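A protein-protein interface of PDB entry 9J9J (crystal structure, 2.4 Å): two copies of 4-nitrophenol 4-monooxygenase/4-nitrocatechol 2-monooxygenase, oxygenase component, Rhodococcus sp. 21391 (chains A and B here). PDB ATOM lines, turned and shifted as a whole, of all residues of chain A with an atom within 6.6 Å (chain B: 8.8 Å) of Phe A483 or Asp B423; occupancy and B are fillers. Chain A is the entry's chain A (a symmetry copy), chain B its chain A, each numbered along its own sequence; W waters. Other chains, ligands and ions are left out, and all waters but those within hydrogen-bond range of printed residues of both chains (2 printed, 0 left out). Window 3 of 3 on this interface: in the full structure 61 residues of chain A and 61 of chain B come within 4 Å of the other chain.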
ATOM      1  N   ASP A 475      18.387  30.375 -31.082  1.00  0.00           N
ATOM      2  CA  ASP A 475      17.489  30.744 -32.162  1.00  0.00           C
ATOM      3  C   ASP A 475      16.829  29.504 -32.735  1.00  0.00           C
ATOM      4  O   ASP A 475      15.624  29.503 -32.946  1.00  0.00           O
ATOM      5  CB  ASP A 475      18.203  31.479 -33.283  1.00  0.00           C
ATOM      6  CG  ASP A 475      18.600  32.912 -32.967  1.00  0.00           C
ATOM      7  OD1 ASP A 475      17.966  33.526 -32.080  1.00  0.00           O
ATOM      8  OD2 ASP A 475      19.571  33.388 -33.582  1.00  0.00           O
ATOM      9  N   ALA A 477      16.419  26.585 -31.418  1.00  0.00           N
ATOM     10  CA  ALA A 477      15.503  25.998 -30.466  1.00  0.00           C
ATOM     11  C   ALA A 477      14.229  26.825 -30.376  1.00  0.00           C
ATOM     12  O   ALA A 477      13.140  26.277 -30.324  1.00  0.00           O
ATOM     13  CB  ALA A 477      16.182  25.846 -29.139  1.00  0.00           C
ATOM     14  N   ARG A 478      14.342  28.153 -30.373  1.00  0.00           N
ATOM     15  CA  ARG A 478      13.153  28.966 -30.190  1.00  0.00           C
ATOM     16  C   ARG A 478      12.221  28.794 -31.370  1.00  0.00           C
ATOM     17  O   ARG A 478      11.010  28.780 -31.227  1.00  0.00           O
ATOM     18  CB  ARG A 478      13.484  30.451 -30.081  1.00  0.00           C
ATOM     19  CG  ARG A 478      14.033  30.846 -28.726  1.00  0.00           C
ATOM     20  CD  ARG A 478      14.442  32.300 -28.779  1.00  0.00           C
ATOM     21  NE  ARG A 478      15.228  32.655 -27.602  1.00  0.00           N
ATOM     22  CZ  ARG A 478      14.828  32.725 -26.319  1.00  0.00           C
ATOM     23  NH1 ARG A 478      13.546  32.804 -25.982  1.00  0.00           N
ATOM     24  NH2 ARG A 478      15.746  32.799 -25.368  1.00  0.00           N
ATOM     25  N   GLN A 479      12.808  28.719 -32.545  1.00  0.00           N
ATOM     26  CA  GLN A 479      12.042  28.571 -33.768  1.00  0.00           C
ATOM     27  C   GLN A 479      11.283  27.245 -33.754  1.00  0.00           C
ATOM     28  O   GLN A 479      10.125  27.193 -34.130  1.00  0.00           O
ATOM     29  CB  GLN A 479      13.082  28.739 -34.875  1.00  0.00           C
ATOM     30  CG  GLN A 479      12.565  28.531 -36.288  1.00  0.00           C
ATOM     31  CD  GLN A 479      13.668  28.738 -37.302  1.00  0.00           C
ATOM     32  OE1 GLN A 479      14.315  29.793 -37.341  1.00  0.00           O
ATOM     33  NE2 GLN A 479      13.941  27.706 -38.085  1.00  0.00           N
ATOM     34  N   VAL A 480      11.926  26.169 -33.308  1.00  0.00           N
ATOM     35  CA  VAL A 480      11.264  24.885 -33.199  1.00  0.00           C
ATOM     36  C   VAL A 480      10.115  24.951 -32.198  1.00  0.00           C
ATOM     37  O   VAL A 480       9.085  24.318 -32.384  1.00  0.00           O
ATOM     38  CB  VAL A 480      12.362  23.894 -32.777  1.00  0.00           C
ATOM     39  CG1 VAL A 480      11.858  22.729 -31.955  1.00  0.00           C
ATOM     40  CG2 VAL A 480      13.173  23.412 -33.975  1.00  0.00           C
ATOM     41  N   LEU A 481      10.276  25.698 -31.109  1.00  0.00           N
ATOM     42  CA  LEU A 481       9.238  25.758 -30.093  1.00  0.00           C
ATOM     43  C   LEU A 481       8.192  26.818 -30.425  1.00  0.00           C
ATOM     44  O   LEU A 481       7.162  26.857 -29.765  1.00  0.00           O
ATOM     45  CB  LEU A 481       9.876  26.089 -28.750  1.00  0.00           C
ATOM     46  CG  LEU A 481      10.716  24.985 -28.121  1.00  0.00           C
ATOM     47  CD1 LEU A 481      11.724  25.494 -27.111  1.00  0.00           C
ATOM     48  CD2 LEU A 481       9.766  24.019 -27.467  1.00  0.00           C
ATOM     49  N   GLY A 482       8.458  27.696 -31.393  1.00  0.00           N
ATOM     50  CA  GLY A 482       7.541  28.788 -31.673  1.00  0.00           C
ATOM     51  C   GLY A 482       7.563  29.819 -30.542  1.00  0.00           C
ATOM     52  O   GLY A 482       6.535  30.211 -30.033  1.00  0.00           O
ATOM     53  N   PHE A 483       8.753  30.253 -30.123  1.00  0.00           N
ATOM     54  CA  PHE A 483       8.871  31.157 -28.993  1.00  0.00           C
ATOM     55  C   PHE A 483       9.504  32.464 -29.454  1.00  0.00           C
ATOM     56  O   PHE A 483      10.448  32.460 -30.245  1.00  0.00           O
ATOM     57  CB  PHE A 483       9.797  30.688 -27.860  1.00  0.00           C
ATOM     58  CG  PHE A 483       9.335  29.594 -26.902  1.00  0.00           C
ATOM     59  CD1 PHE A 483       8.021  29.143 -26.876  1.00  0.00           C
ATOM     60  CD2 PHE A 483      10.232  29.042 -25.998  1.00  0.00           C
ATOM     61  CE1 PHE A 483       7.647  28.136 -26.012  1.00  0.00           C
ATOM     62  CE2 PHE A 483       9.835  28.061 -25.111  1.00  0.00           C
ATOM     63  CZ  PHE A 483       8.551  27.603 -25.134  1.00  0.00           C
ATOM     64  N   GLY A 484       9.025  33.574 -28.889  1.00  0.00           N
ATOM     65  CA  GLY A 484       9.790  34.804 -28.948  1.00  0.00           C
ATOM     66  C   GLY A 484      11.020  34.690 -28.055  1.00  0.00           C
ATOM     67  O   GLY A 484      11.492  33.586 -27.801  1.00  0.00           O
ATOM     68  N   ASP A 485      11.527  35.840 -27.596  1.00  0.00           N
ATOM     69  CA  ASP A 485      12.651  35.944 -26.669  1.00  0.00           C
ATOM     70  C   ASP A 485      12.128  35.857 -25.230  1.00  0.00           C
ATOM     71  O   ASP A 485      10.918  35.765 -25.032  1.00  0.00           O
ATOM     72  CB  ASP A 485      13.445  37.221 -26.945  1.00  0.00           C
ATOM     73  CG  ASP A 485      12.730  38.543 -26.666  1.00  0.00           C
ATOM     74  OD1 ASP A 485      11.508  38.643 -26.934  1.00  0.00           O
ATOM     75  OD2 ASP A 485      13.401  39.467 -26.178  1.00  0.00           O
ATOM     76  N   ALA A 488       9.280  38.151 -24.551  1.00  0.00           N
ATOM     77  CA  ALA A 488       8.031  37.775 -25.182  1.00  0.00           C
ATOM     78  C   ALA A 488       7.350  36.689 -24.360  1.00  0.00           C
ATOM     79  O   ALA A 488       6.151  36.762 -24.140  1.00  0.00           O
ATOM     80  CB  ALA A 488       8.293  37.306 -26.597  1.00  0.00           C
ATOM     81  N   LEU A 489       8.131  35.687 -23.921  1.00  0.00           N
ATOM     82  CA  LEU A 489       7.615  34.557 -23.157  1.00  0.00           C
ATOM     83  C   LEU A 489       7.106  34.997 -21.790  1.00  0.00           C
ATOM     84  O   LEU A 489       6.093  34.485 -21.332  1.00  0.00           O
ATOM     85  CB  LEU A 489       8.711  33.514 -22.959  1.00  0.00           C
ATOM     86  CG  LEU A 489       9.010  32.625 -24.161  1.00  0.00           C
ATOM     87  CD1 LEU A 489      10.346  31.932 -23.998  1.00  0.00           C
ATOM     88  CD2 LEU A 489       7.875  31.636 -24.271  1.00  0.00           C
ATOM     89  N   ARG A 492       3.722  36.578 -22.102  1.00  0.00           N
ATOM     90  CA  ARG A 492       2.579  35.682 -22.211  1.00  0.00           C
ATOM     91  C   ARG A 492       2.216  35.140 -20.827  1.00  0.00           C
ATOM     92  O   ARG A 492       1.049  35.092 -20.454  1.00  0.00           O
ATOM     93  CB  ARG A 492       2.796  34.510 -23.175  1.00  0.00           C
ATOM     94  CG  ARG A 492       1.691  33.454 -23.060  1.00  0.00           C
ATOM     95  CD  ARG A 492       1.849  32.182 -23.898  1.00  0.00           C
ATOM     96  NE  ARG A 492       2.028  32.546 -25.304  1.00  0.00           N
ATOM     97  CZ  ARG A 492       3.202  32.667 -25.903  1.00  0.00           C
ATOM     98  NH1 ARG A 492       4.256  32.013 -25.466  1.00  0.00           N
ATOM     99  NH2 ARG A 492       3.299  33.402 -26.989  1.00  0.00           N
ATOM    100  N   ALA A 493       3.230  34.711 -20.071  1.00  0.00           N
ATOM    101  CA  ALA A 493       3.018  34.150 -18.751  1.00  0.00           C
ATOM    102  C   ALA A 493       2.250  35.138 -17.877  1.00  0.00           C
ATOM    103  O   ALA A 493       1.289  34.762 -17.206  1.00  0.00           O
ATOM    104  CB  ALA A 493       4.351  33.809 -18.129  1.00  0.00           C
ATOM    105  N   TYR B 245       0.232  19.845 -29.902  1.00  0.00           N
ATOM    106  CA  TYR B 245       0.783  20.243 -28.608  1.00  0.00           C
ATOM    107  C   TYR B 245       1.365  19.020 -27.907  1.00  0.00           C
ATOM    108  O   TYR B 245       2.427  19.097 -27.305  1.00  0.00           O
ATOM    109  CB  TYR B 245      -0.249  20.951 -27.729  1.00  0.00           C
ATOM    110  CG  TYR B 245       0.350  21.407 -26.424  1.00  0.00           C
ATOM    111  CD1 TYR B 245       0.364  20.557 -25.344  1.00  0.00           C
ATOM    112  CD2 TYR B 245       0.937  22.650 -26.280  1.00  0.00           C
ATOM    113  CE1 TYR B 245       0.934  20.924 -24.145  1.00  0.00           C
ATOM    114  CE2 TYR B 245       1.527  23.018 -25.083  1.00  0.00           C
ATOM    115  CZ  TYR B 245       1.525  22.155 -24.006  1.00  0.00           C
ATOM    116  OH  TYR B 245       2.072  22.431 -22.773  1.00  0.00           O
ATOM    117  N   GLY B 309      20.660  24.628 -27.350  1.00  0.00           N
ATOM    118  CA  GLY B 309      19.592  25.629 -27.329  1.00  0.00           C
ATOM    119  C   GLY B 309      18.462  25.218 -26.395  1.00  0.00           C
ATOM    120  O   GLY B 309      18.053  25.984 -25.516  1.00  0.00           O
ATOM    121  N   LEU B 310      17.980  23.978 -26.565  1.00  0.00           N
ATOM    122  CA  LEU B 310      16.895  23.490 -25.736  1.00  0.00           C
ATOM    123  C   LEU B 310      17.321  23.511 -24.269  1.00  0.00           C
ATOM    124  O   LEU B 310      16.522  23.763 -23.367  1.00  0.00           O
ATOM    125  CB  LEU B 310      16.518  22.082 -26.175  1.00  0.00           C
ATOM    126  CG  LEU B 310      15.733  21.944 -27.474  1.00  0.00           C
ATOM    127  CD1 LEU B 310      15.613  20.499 -27.807  1.00  0.00           C
ATOM    128  CD2 LEU B 310      14.363  22.565 -27.358  1.00  0.00           C
ATOM    129  N   LEU B 313      17.128  26.991 -22.822  1.00  0.00           N
ATOM    130  CA  LEU B 313      15.762  27.432 -22.594  1.00  0.00           C
ATOM    131  C   LEU B 313      15.219  26.703 -21.381  1.00  0.00           C
ATOM    132  O   LEU B 313      14.571  27.307 -20.529  1.00  0.00           O
ATOM    133  CB  LEU B 313      14.881  27.170 -23.819  1.00  0.00           C
ATOM    134  CG  LEU B 313      15.141  28.079 -25.022  1.00  0.00           C
ATOM    135  CD1 LEU B 313      14.579  27.506 -26.297  1.00  0.00           C
ATOM    136  CD2 LEU B 313      14.563  29.463 -24.800  1.00  0.00           C
ATOM    137  N   LEU B 314      15.489  25.390 -21.341  1.00  0.00           N
ATOM    138  CA  LEU B 314      14.967  24.547 -20.289  1.00  0.00           C
ATOM    139  C   LEU B 314      15.474  24.995 -18.923  1.00  0.00           C
ATOM    140  O   LEU B 314      14.689  25.121 -17.990  1.00  0.00           O
ATOM    141  CB  LEU B 314      15.353  23.106 -20.562  1.00  0.00           C
ATOM    142  CG  LEU B 314      14.924  22.125 -19.485  1.00  0.00           C
ATOM    143  CD1 LEU B 314      13.428  21.985 -19.396  1.00  0.00           C
ATOM    144  CD2 LEU B 314      15.575  20.808 -19.776  1.00  0.00           C
ATOM    145  N   ALA B 317      14.038  28.194 -18.019  1.00  0.00           N
ATOM    146  CA  ALA B 317      12.641  28.126 -17.644  1.00  0.00           C
ATOM    147  C   ALA B 317      12.462  27.529 -16.252  1.00  0.00           C
ATOM    148  O   ALA B 317      11.467  27.781 -15.599  1.00  0.00           O
ATOM    149  CB  ALA B 317      11.904  27.330 -18.682  1.00  0.00           C
ATOM    150  N   PHE B 401      -4.805  20.349 -19.781  1.00  0.00           N
ATOM    151  CA  PHE B 401      -4.825  21.784 -19.553  1.00  0.00           C
ATOM    152  C   PHE B 401      -6.170  22.381 -19.977  1.00  0.00           C
ATOM    153  O   PHE B 401      -6.559  23.406 -19.465  1.00  0.00           O
ATOM    154  CB  PHE B 401      -3.711  22.482 -20.328  1.00  0.00           C
ATOM    155  CG  PHE B 401      -2.317  22.467 -19.730  1.00  0.00           C
ATOM    156  CD1 PHE B 401      -2.083  22.895 -18.435  1.00  0.00           C
ATOM    157  CD2 PHE B 401      -1.231  22.044 -20.487  1.00  0.00           C
ATOM    158  CE1 PHE B 401      -0.801  22.891 -17.903  1.00  0.00           C
ATOM    159  CE2 PHE B 401       0.039  22.041 -19.958  1.00  0.00           C
ATOM    160  CZ  PHE B 401       0.258  22.478 -18.669  1.00  0.00           C
ATOM    161  N   GLU B 411      -2.365  25.040 -14.912  1.00  0.00           N
ATOM    162  CA  GLU B 411      -1.677  26.200 -15.433  1.00  0.00           C
ATOM    163  C   GLU B 411      -1.096  26.962 -14.263  1.00  0.00           C
ATOM    164  O   GLU B 411      -0.078  27.630 -14.408  1.00  0.00           O
ATOM    165  CB  GLU B 411      -2.626  27.107 -16.216  1.00  0.00           C
ATOM    166  CG  GLU B 411      -3.162  26.439 -17.476  1.00  0.00           C
ATOM    167  CD  GLU B 411      -3.964  27.360 -18.371  1.00  0.00           C
ATOM    168  OE1 GLU B 411      -4.930  27.950 -17.881  1.00  0.00           O
ATOM    169  OE2 GLU B 411      -3.659  27.449 -19.562  1.00  0.00           O
ATOM    170  N   LEU B 414       1.858  24.428 -12.499  1.00  0.00           N
ATOM    171  CA  LEU B 414       3.059  24.065 -13.235  1.00  0.00           C
ATOM    172  C   LEU B 414       3.734  25.259 -13.891  1.00  0.00           C
ATOM    173  O   LEU B 414       4.666  25.039 -14.657  1.00  0.00           O
ATOM    174  CB  LEU B 414       2.714  23.035 -14.303  1.00  0.00           C
ATOM    175  CG  LEU B 414       2.112  21.742 -13.773  1.00  0.00           C
ATOM    176  CD1 LEU B 414       2.033  20.666 -14.829  1.00  0.00           C
ATOM    177  CD2 LEU B 414       2.955  21.295 -12.602  1.00  0.00           C
ATOM    178  N   ARG B 415       3.278  26.494 -13.632  1.00  0.00           N
ATOM    179  CA  ARG B 415       3.906  27.658 -14.242  1.00  0.00           C
ATOM    180  C   ARG B 415       5.225  27.990 -13.560  1.00  0.00           C
ATOM    181  O   ARG B 415       5.491  27.562 -12.452  1.00  0.00           O
ATOM    182  CB  ARG B 415       3.110  28.958 -14.159  1.00  0.00           C
ATOM    183  CG  ARG B 415       3.001  29.481 -12.742  1.00  0.00           C
ATOM    184  CD  ARG B 415       2.035  30.641 -12.650  1.00  0.00           C
ATOM    185  NE  ARG B 415       1.442  30.569 -11.312  1.00  0.00           N
ATOM    186  CZ  ARG B 415       1.610  31.450 -10.358  1.00  0.00           C
ATOM    187  NH1 ARG B 415       2.308  32.538 -10.591  1.00  0.00           N
ATOM    188  NH2 ARG B 415       1.060  31.258  -9.180  1.00  0.00           N
ATOM    189  N   GLY B 416       6.037  28.788 -14.248  1.00  0.00           N
ATOM    190  CA  GLY B 416       7.258  29.327 -13.687  1.00  0.00           C
ATOM    191  C   GLY B 416       7.144  30.836 -13.536  1.00  0.00           C
ATOM    192  O   GLY B 416       6.150  31.447 -13.949  1.00  0.00           O
ATOM    193  N   SER B 418       8.493  33.174 -15.069  1.00  0.00           N
ATOM    194  CA  SER B 418       8.525  33.997 -16.257  1.00  0.00           C
ATOM    195  C   SER B 418       8.179  33.156 -17.475  1.00  0.00           C
ATOM    196  O   SER B 418       8.589  33.496 -18.582  1.00  0.00           O
ATOM    197  CB  SER B 418       9.888  34.644 -16.415  1.00  0.00           C
ATOM    198  OG  SER B 418      10.289  35.348 -15.242  1.00  0.00           O
ATOM    199  N   ILE B 419       7.418  32.075 -17.272  1.00  0.00           N
ATOM    200  CA  ILE B 419       6.966  31.267 -18.391  1.00  0.00           C
ATOM    201  C   ILE B 419       5.718  30.533 -17.948  1.00  0.00           C
ATOM    202  O   ILE B 419       5.666  30.079 -16.822  1.00  0.00           O
ATOM    203  CB  ILE B 419       8.062  30.293 -18.863  1.00  0.00           C
ATOM    204  CG1 ILE B 419       7.574  29.448 -20.012  1.00  0.00           C
ATOM    205  CG2 ILE B 419       8.535  29.400 -17.727  1.00  0.00           C
ATOM    206  CD1 ILE B 419       8.643  28.628 -20.688  1.00  0.00           C
ATOM    207  N   SER B 420       4.703  30.466 -18.806  1.00  0.00           N
ATOM    208  CA  SER B 420       3.461  29.788 -18.464  1.00  0.00           C
ATOM    209  C   SER B 420       3.660  28.278 -18.364  1.00  0.00           C
ATOM    210  O   SER B 420       4.652  27.722 -18.836  1.00  0.00           O
ATOM    211  CB  SER B 420       2.424  30.065 -19.490  1.00  0.00           C
ATOM    212  OG  SER B 420       2.798  29.447 -20.711  1.00  0.00           O
ATOM    213  N   ALA B 421       2.657  27.606 -17.807  1.00  0.00           N
ATOM    214  CA  ALA B 421       2.702  26.172 -17.649  1.00  0.00           C
ATOM    215  C   ALA B 421       2.809  25.493 -19.000  1.00  0.00           C
ATOM    216  O   ALA B 421       3.556  24.527 -19.146  1.00  0.00           O
ATOM    217  CB  ALA B 421       1.466  25.721 -16.970  1.00  0.00           C
ATOM    218  N   ARG B 422       2.018  25.990 -19.953  1.00  0.00           N
ATOM    219  CA  ARG B 422       1.870  25.370 -21.250  1.00  0.00           C
ATOM    220  C   ARG B 422       3.183  25.486 -22.020  1.00  0.00           C
ATOM    221  O   ARG B 422       3.642  24.548 -22.652  1.00  0.00           O
ATOM    222  CB  ARG B 422       0.720  26.015 -22.029  1.00  0.00           C
ATOM    223  CG  ARG B 422      -0.671  25.682 -21.514  1.00  0.00           C
ATOM    224  CD  ARG B 422      -1.742  26.339 -22.373  1.00  0.00           C
ATOM    225  NE  ARG B 422      -3.108  26.183 -21.857  1.00  0.00           N
ATOM    226  CZ  ARG B 422      -4.107  25.420 -22.339  1.00  0.00           C
ATOM    227  NH1 ARG B 422      -3.982  24.704 -23.423  1.00  0.00           N
ATOM    228  NH2 ARG B 422      -5.280  25.389 -21.747  1.00  0.00           N
ATOM    229  N   ASP B 423       3.758  26.680 -22.018  1.00  0.00           N
ATOM    230  CA  ASP B 423       4.976  26.914 -22.754  1.00  0.00           C
ATOM    231  C   ASP B 423       6.079  26.036 -22.183  1.00  0.00           C
ATOM    232  O   ASP B 423       6.817  25.430 -22.935  1.00  0.00           O
ATOM    233  CB  ASP B 423       5.344  28.376 -22.670  1.00  0.00           C
ATOM    234  CG  ASP B 423       4.534  29.286 -23.568  1.00  0.00           C
ATOM    235  OD1 ASP B 423       3.861  28.765 -24.458  1.00  0.00           O
ATOM    236  OD2 ASP B 423       4.622  30.501 -23.367  1.00  0.00           O
ATOM    237  N   ARG B 424       6.190  25.982 -20.853  1.00  0.00           N
ATOM    238  CA  ARG B 424       7.241  25.223 -20.206  1.00  0.00           C
ATOM    239  C   ARG B 424       7.048  23.734 -20.473  1.00  0.00           C
ATOM    240  O   ARG B 424       8.010  23.029 -20.767  1.00  0.00           O
ATOM    241  CB  ARG B 424       7.303  25.526 -18.704  1.00  0.00           C
ATOM    242  CG  ARG B 424       8.532  24.862 -18.106  1.00  0.00           C
ATOM    243  CD  ARG B 424       9.011  25.416 -16.802  1.00  0.00           C
ATOM    244  NE  ARG B 424       8.085  25.166 -15.701  1.00  0.00           N
ATOM    245  CZ  ARG B 424       8.320  25.566 -14.457  1.00  0.00           C
ATOM    246  NH1 ARG B 424       9.415  26.234 -14.185  1.00  0.00           N
ATOM    247  NH2 ARG B 424       7.450  25.335 -13.499  1.00  0.00           N
ATOM    248  N   VAL B 425       5.815  23.245 -20.436  1.00  0.00           N
ATOM    249  CA  VAL B 425       5.606  21.826 -20.683  1.00  0.00           C
ATOM    250  C   VAL B 425       5.893  21.511 -22.154  1.00  0.00           C
ATOM    251  O   VAL B 425       6.298  20.405 -22.523  1.00  0.00           O
ATOM    252  CB  VAL B 425       4.195  21.460 -20.228  1.00  0.00           C
ATOM    253  CG1 VAL B 425       3.728  20.129 -20.771  1.00  0.00           C
ATOM    254  CG2 VAL B 425       4.117  21.459 -18.710  1.00  0.00           C
ATOM    255  N   SER B 426       5.784  22.517 -23.011  1.00  0.00           N
ATOM    256  CA  SER B 426       6.065  22.264 -24.408  1.00  0.00           C
ATOM    257  C   SER B 426       7.558  22.045 -24.591  1.00  0.00           C
ATOM    258  O   SER B 426       7.953  21.452 -25.582  1.00  0.00           O
ATOM    259  CB  SER B 426       5.515  23.378 -25.321  1.00  0.00           C
ATOM    260  OG  SER B 426       6.333  24.529 -25.213  1.00  0.00           O
ATOM    261  N   ILE B 427       8.392  22.515 -23.652  1.00  0.00           N
ATOM    262  CA  ILE B 427       9.812  22.264 -23.773  1.00  0.00           C
ATOM    263  C   ILE B 427      10.075  20.802 -23.435  1.00  0.00           C
ATOM    264  O   ILE B 427      10.816  20.117 -24.121  1.00  0.00           O
ATOM    265  CB  ILE B 427      10.671  23.186 -22.904  1.00  0.00           C
ATOM    266  CG1 ILE B 427      10.377  24.673 -23.110  1.00  0.00           C
ATOM    267  CG2 ILE B 427      12.143  22.899 -23.196  1.00  0.00           C
ATOM    268  CD1 ILE B 427      11.162  25.577 -22.161  1.00  0.00           C
ATOM    269  N   PHE B 428       9.458  20.333 -22.366  1.00  0.00           N
ATOM    270  CA  PHE B 428       9.577  18.943 -21.983  1.00  0.00           C
ATOM    271  C   PHE B 428       9.123  18.062 -23.142  1.00  0.00           C
ATOM    272  O   PHE B 428       9.835  17.151 -23.536  1.00  0.00           O
ATOM    273  CB  PHE B 428       8.779  18.691 -20.706  1.00  0.00           C
ATOM    274  CG  PHE B 428       9.234  19.381 -19.428  1.00  0.00           C
ATOM    275  CD1 PHE B 428      10.523  19.279 -18.967  1.00  0.00           C
ATOM    276  CD2 PHE B 428       8.314  20.039 -18.619  1.00  0.00           C
ATOM    277  CE1 PHE B 428      10.897  19.869 -17.764  1.00  0.00           C
ATOM    278  CE2 PHE B 428       8.695  20.644 -17.433  1.00  0.00           C
ATOM    279  CZ  PHE B 428       9.992  20.551 -17.010  1.00  0.00           C
ATOM    280  N   ARG B 429       7.955  18.361 -23.708  1.00  0.00           N
ATOM    281  CA  ARG B 429       7.369  17.517 -24.736  1.00  0.00           C
ATOM    282  C   ARG B 429       8.217  17.485 -26.007  1.00  0.00           C
ATOM    283  O   ARG B 429       8.292  16.454 -26.678  1.00  0.00           O
ATOM    284  CB  ARG B 429       5.963  18.015 -25.047  1.00  0.00           C
ATOM    285  CG  ARG B 429       4.982  17.391 -24.075  1.00  0.00           C
ATOM    286  CD  ARG B 429       3.558  17.785 -24.330  1.00  0.00           C
ATOM    287  NE  ARG B 429       2.700  17.052 -23.401  1.00  0.00           N
ATOM    288  CZ  ARG B 429       2.379  15.794 -23.556  1.00  0.00           C
ATOM    289  NH1 ARG B 429       2.719  15.149 -24.663  1.00  0.00           N
ATOM    290  NH2 ARG B 429       1.688  15.206 -22.610  1.00  0.00           N
ATOM    291  N   GLN B 430       8.885  18.593 -26.319  1.00  0.00           N
ATOM    292  CA  GLN B 430       9.796  18.617 -27.459  1.00  0.00           C
ATOM    293  C   GLN B 430      10.995  17.706 -27.192  1.00  0.00           C
ATOM    294  O   GLN B 430      11.475  17.026 -28.092  1.00  0.00           O
ATOM    295  CB  GLN B 430      10.197  20.073 -27.656  1.00  0.00           C
ATOM    296  CG  GLN B 430      11.184  20.352 -28.768  1.00  0.00           C
ATOM    297  CD  GLN B 430      10.631  20.227 -30.175  1.00  0.00           C
ATOM    298  OE1 GLN B 430      11.364  19.872 -31.105  1.00  0.00           O
ATOM    299  NE2 GLN B 430       9.385  20.616 -30.375  1.00  0.00           N
HETATM  300  O   HOH W   1       8.499  21.783 -33.157  1.00  0.00           O
HETATM  301  O   HOH W   2       5.349  31.742 -21.250  1.00  0.00           O
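Water W2 lies within hydrogen-bond range of OD2 of Asp B423 (2.6 Å), N of Ser B420 (2.8 Å) and O of Leu A489 (2.8 Å).
Water W1 bridges O of Val A480 (2.7 Å) and NE2 of Gln B430 (3.1 Å).
Of the 14 printed residues of chain A, 8 touch a printed residue of chain B.
Hydrophobic or aromatic side chains of chain A that line the printed part of chain B: Ala A477, Val A480, Leu A481, Phe A483, Leu A489 and Ala A493.
Among the printed residues, pairs that only touch across the chains: Ala A477 with Gly B309 (3.6 Å), Ala A477 with Leu B310 (3.7 Å), Ala A477 with Leu B313 (3.7 Å), Arg A478 with Leu B313 (3.6 Å), Val A480 with Gln B430 (3.0 Å), Leu A481 with Leu B310 (3.95 Å), Leu A481 with Leu B313 (3.6 Å), Leu A481 with Ser B426 (3.7 Å), Leu A481 with Gln B430 (3.97 Å), Phe A483 with Asp B423 (3.5 Å), Phe A483 with Ser B426 (3.8 Å), Phe A483 with Ile B427 (3.97 Å), Leu A489 with Ser B418 (3.8 Å), Leu A489 with Asp B423 (3.6 Å), Ala A493 with Ser B418 (3.9 Å), Ala A493 with Ile B419 (3.6 Å) and Ala A493 with Ser B420 (3.4 Å).
Of chain B, only Asp B423, Ser B426 and Ile B427 come within 4 Å of Phe A483.
Of chain A, only Phe A483, Leu A489 and Arg A492 come within 4 Å of Asp B423.
No residue of chain B comes within 4 Å of Gly A482.
No residue of chain B comes within 4 Å of Gly A484.
Of the printed residues of chain A, Leu B313 touches Ala A477 (3.7 Å), Arg A478 (3.6 Å) and Leu A481 (3.6 Å).
Of the printed residues of chain A, Gln B430 touches Val A480 (3.0 Å) and Leu A481 (3.97 Å).
The nearest residue of chain B that does not touch Phe A483 is Leu B313 (4.5 Å).
The nearest residue of chain A that does not touch Asp B423 is Ala A493 (5.5 Å).
The side-chain carboxylate (OD2) of Asp B423 lies within salt-bridge range of the guanidinium group (NH1) of Arg A492, at 2.6 Å.
No position is printed for both chains.
Of the 18 pairs that touch across the chains among the printed residues, none has its exchanged pair printed and touching as well.
The backbone carbonyl oxygen of Asp B423 is in hydrogen-bond range of the side-chain hydroxyl of Ser B426.
The backbone NH of Phe A483 lies within hydrogen-bond range of the backbone carbonyl oxygen of Arg A478 (2.9 Å).
N of Asp B423 is in hydrogen-bond range of OG of Ser B420, 3.2 Å away.
O of Gly A484 sits at hydrogen-bond distance from NH1 of Arg A478 (2.9 Å).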
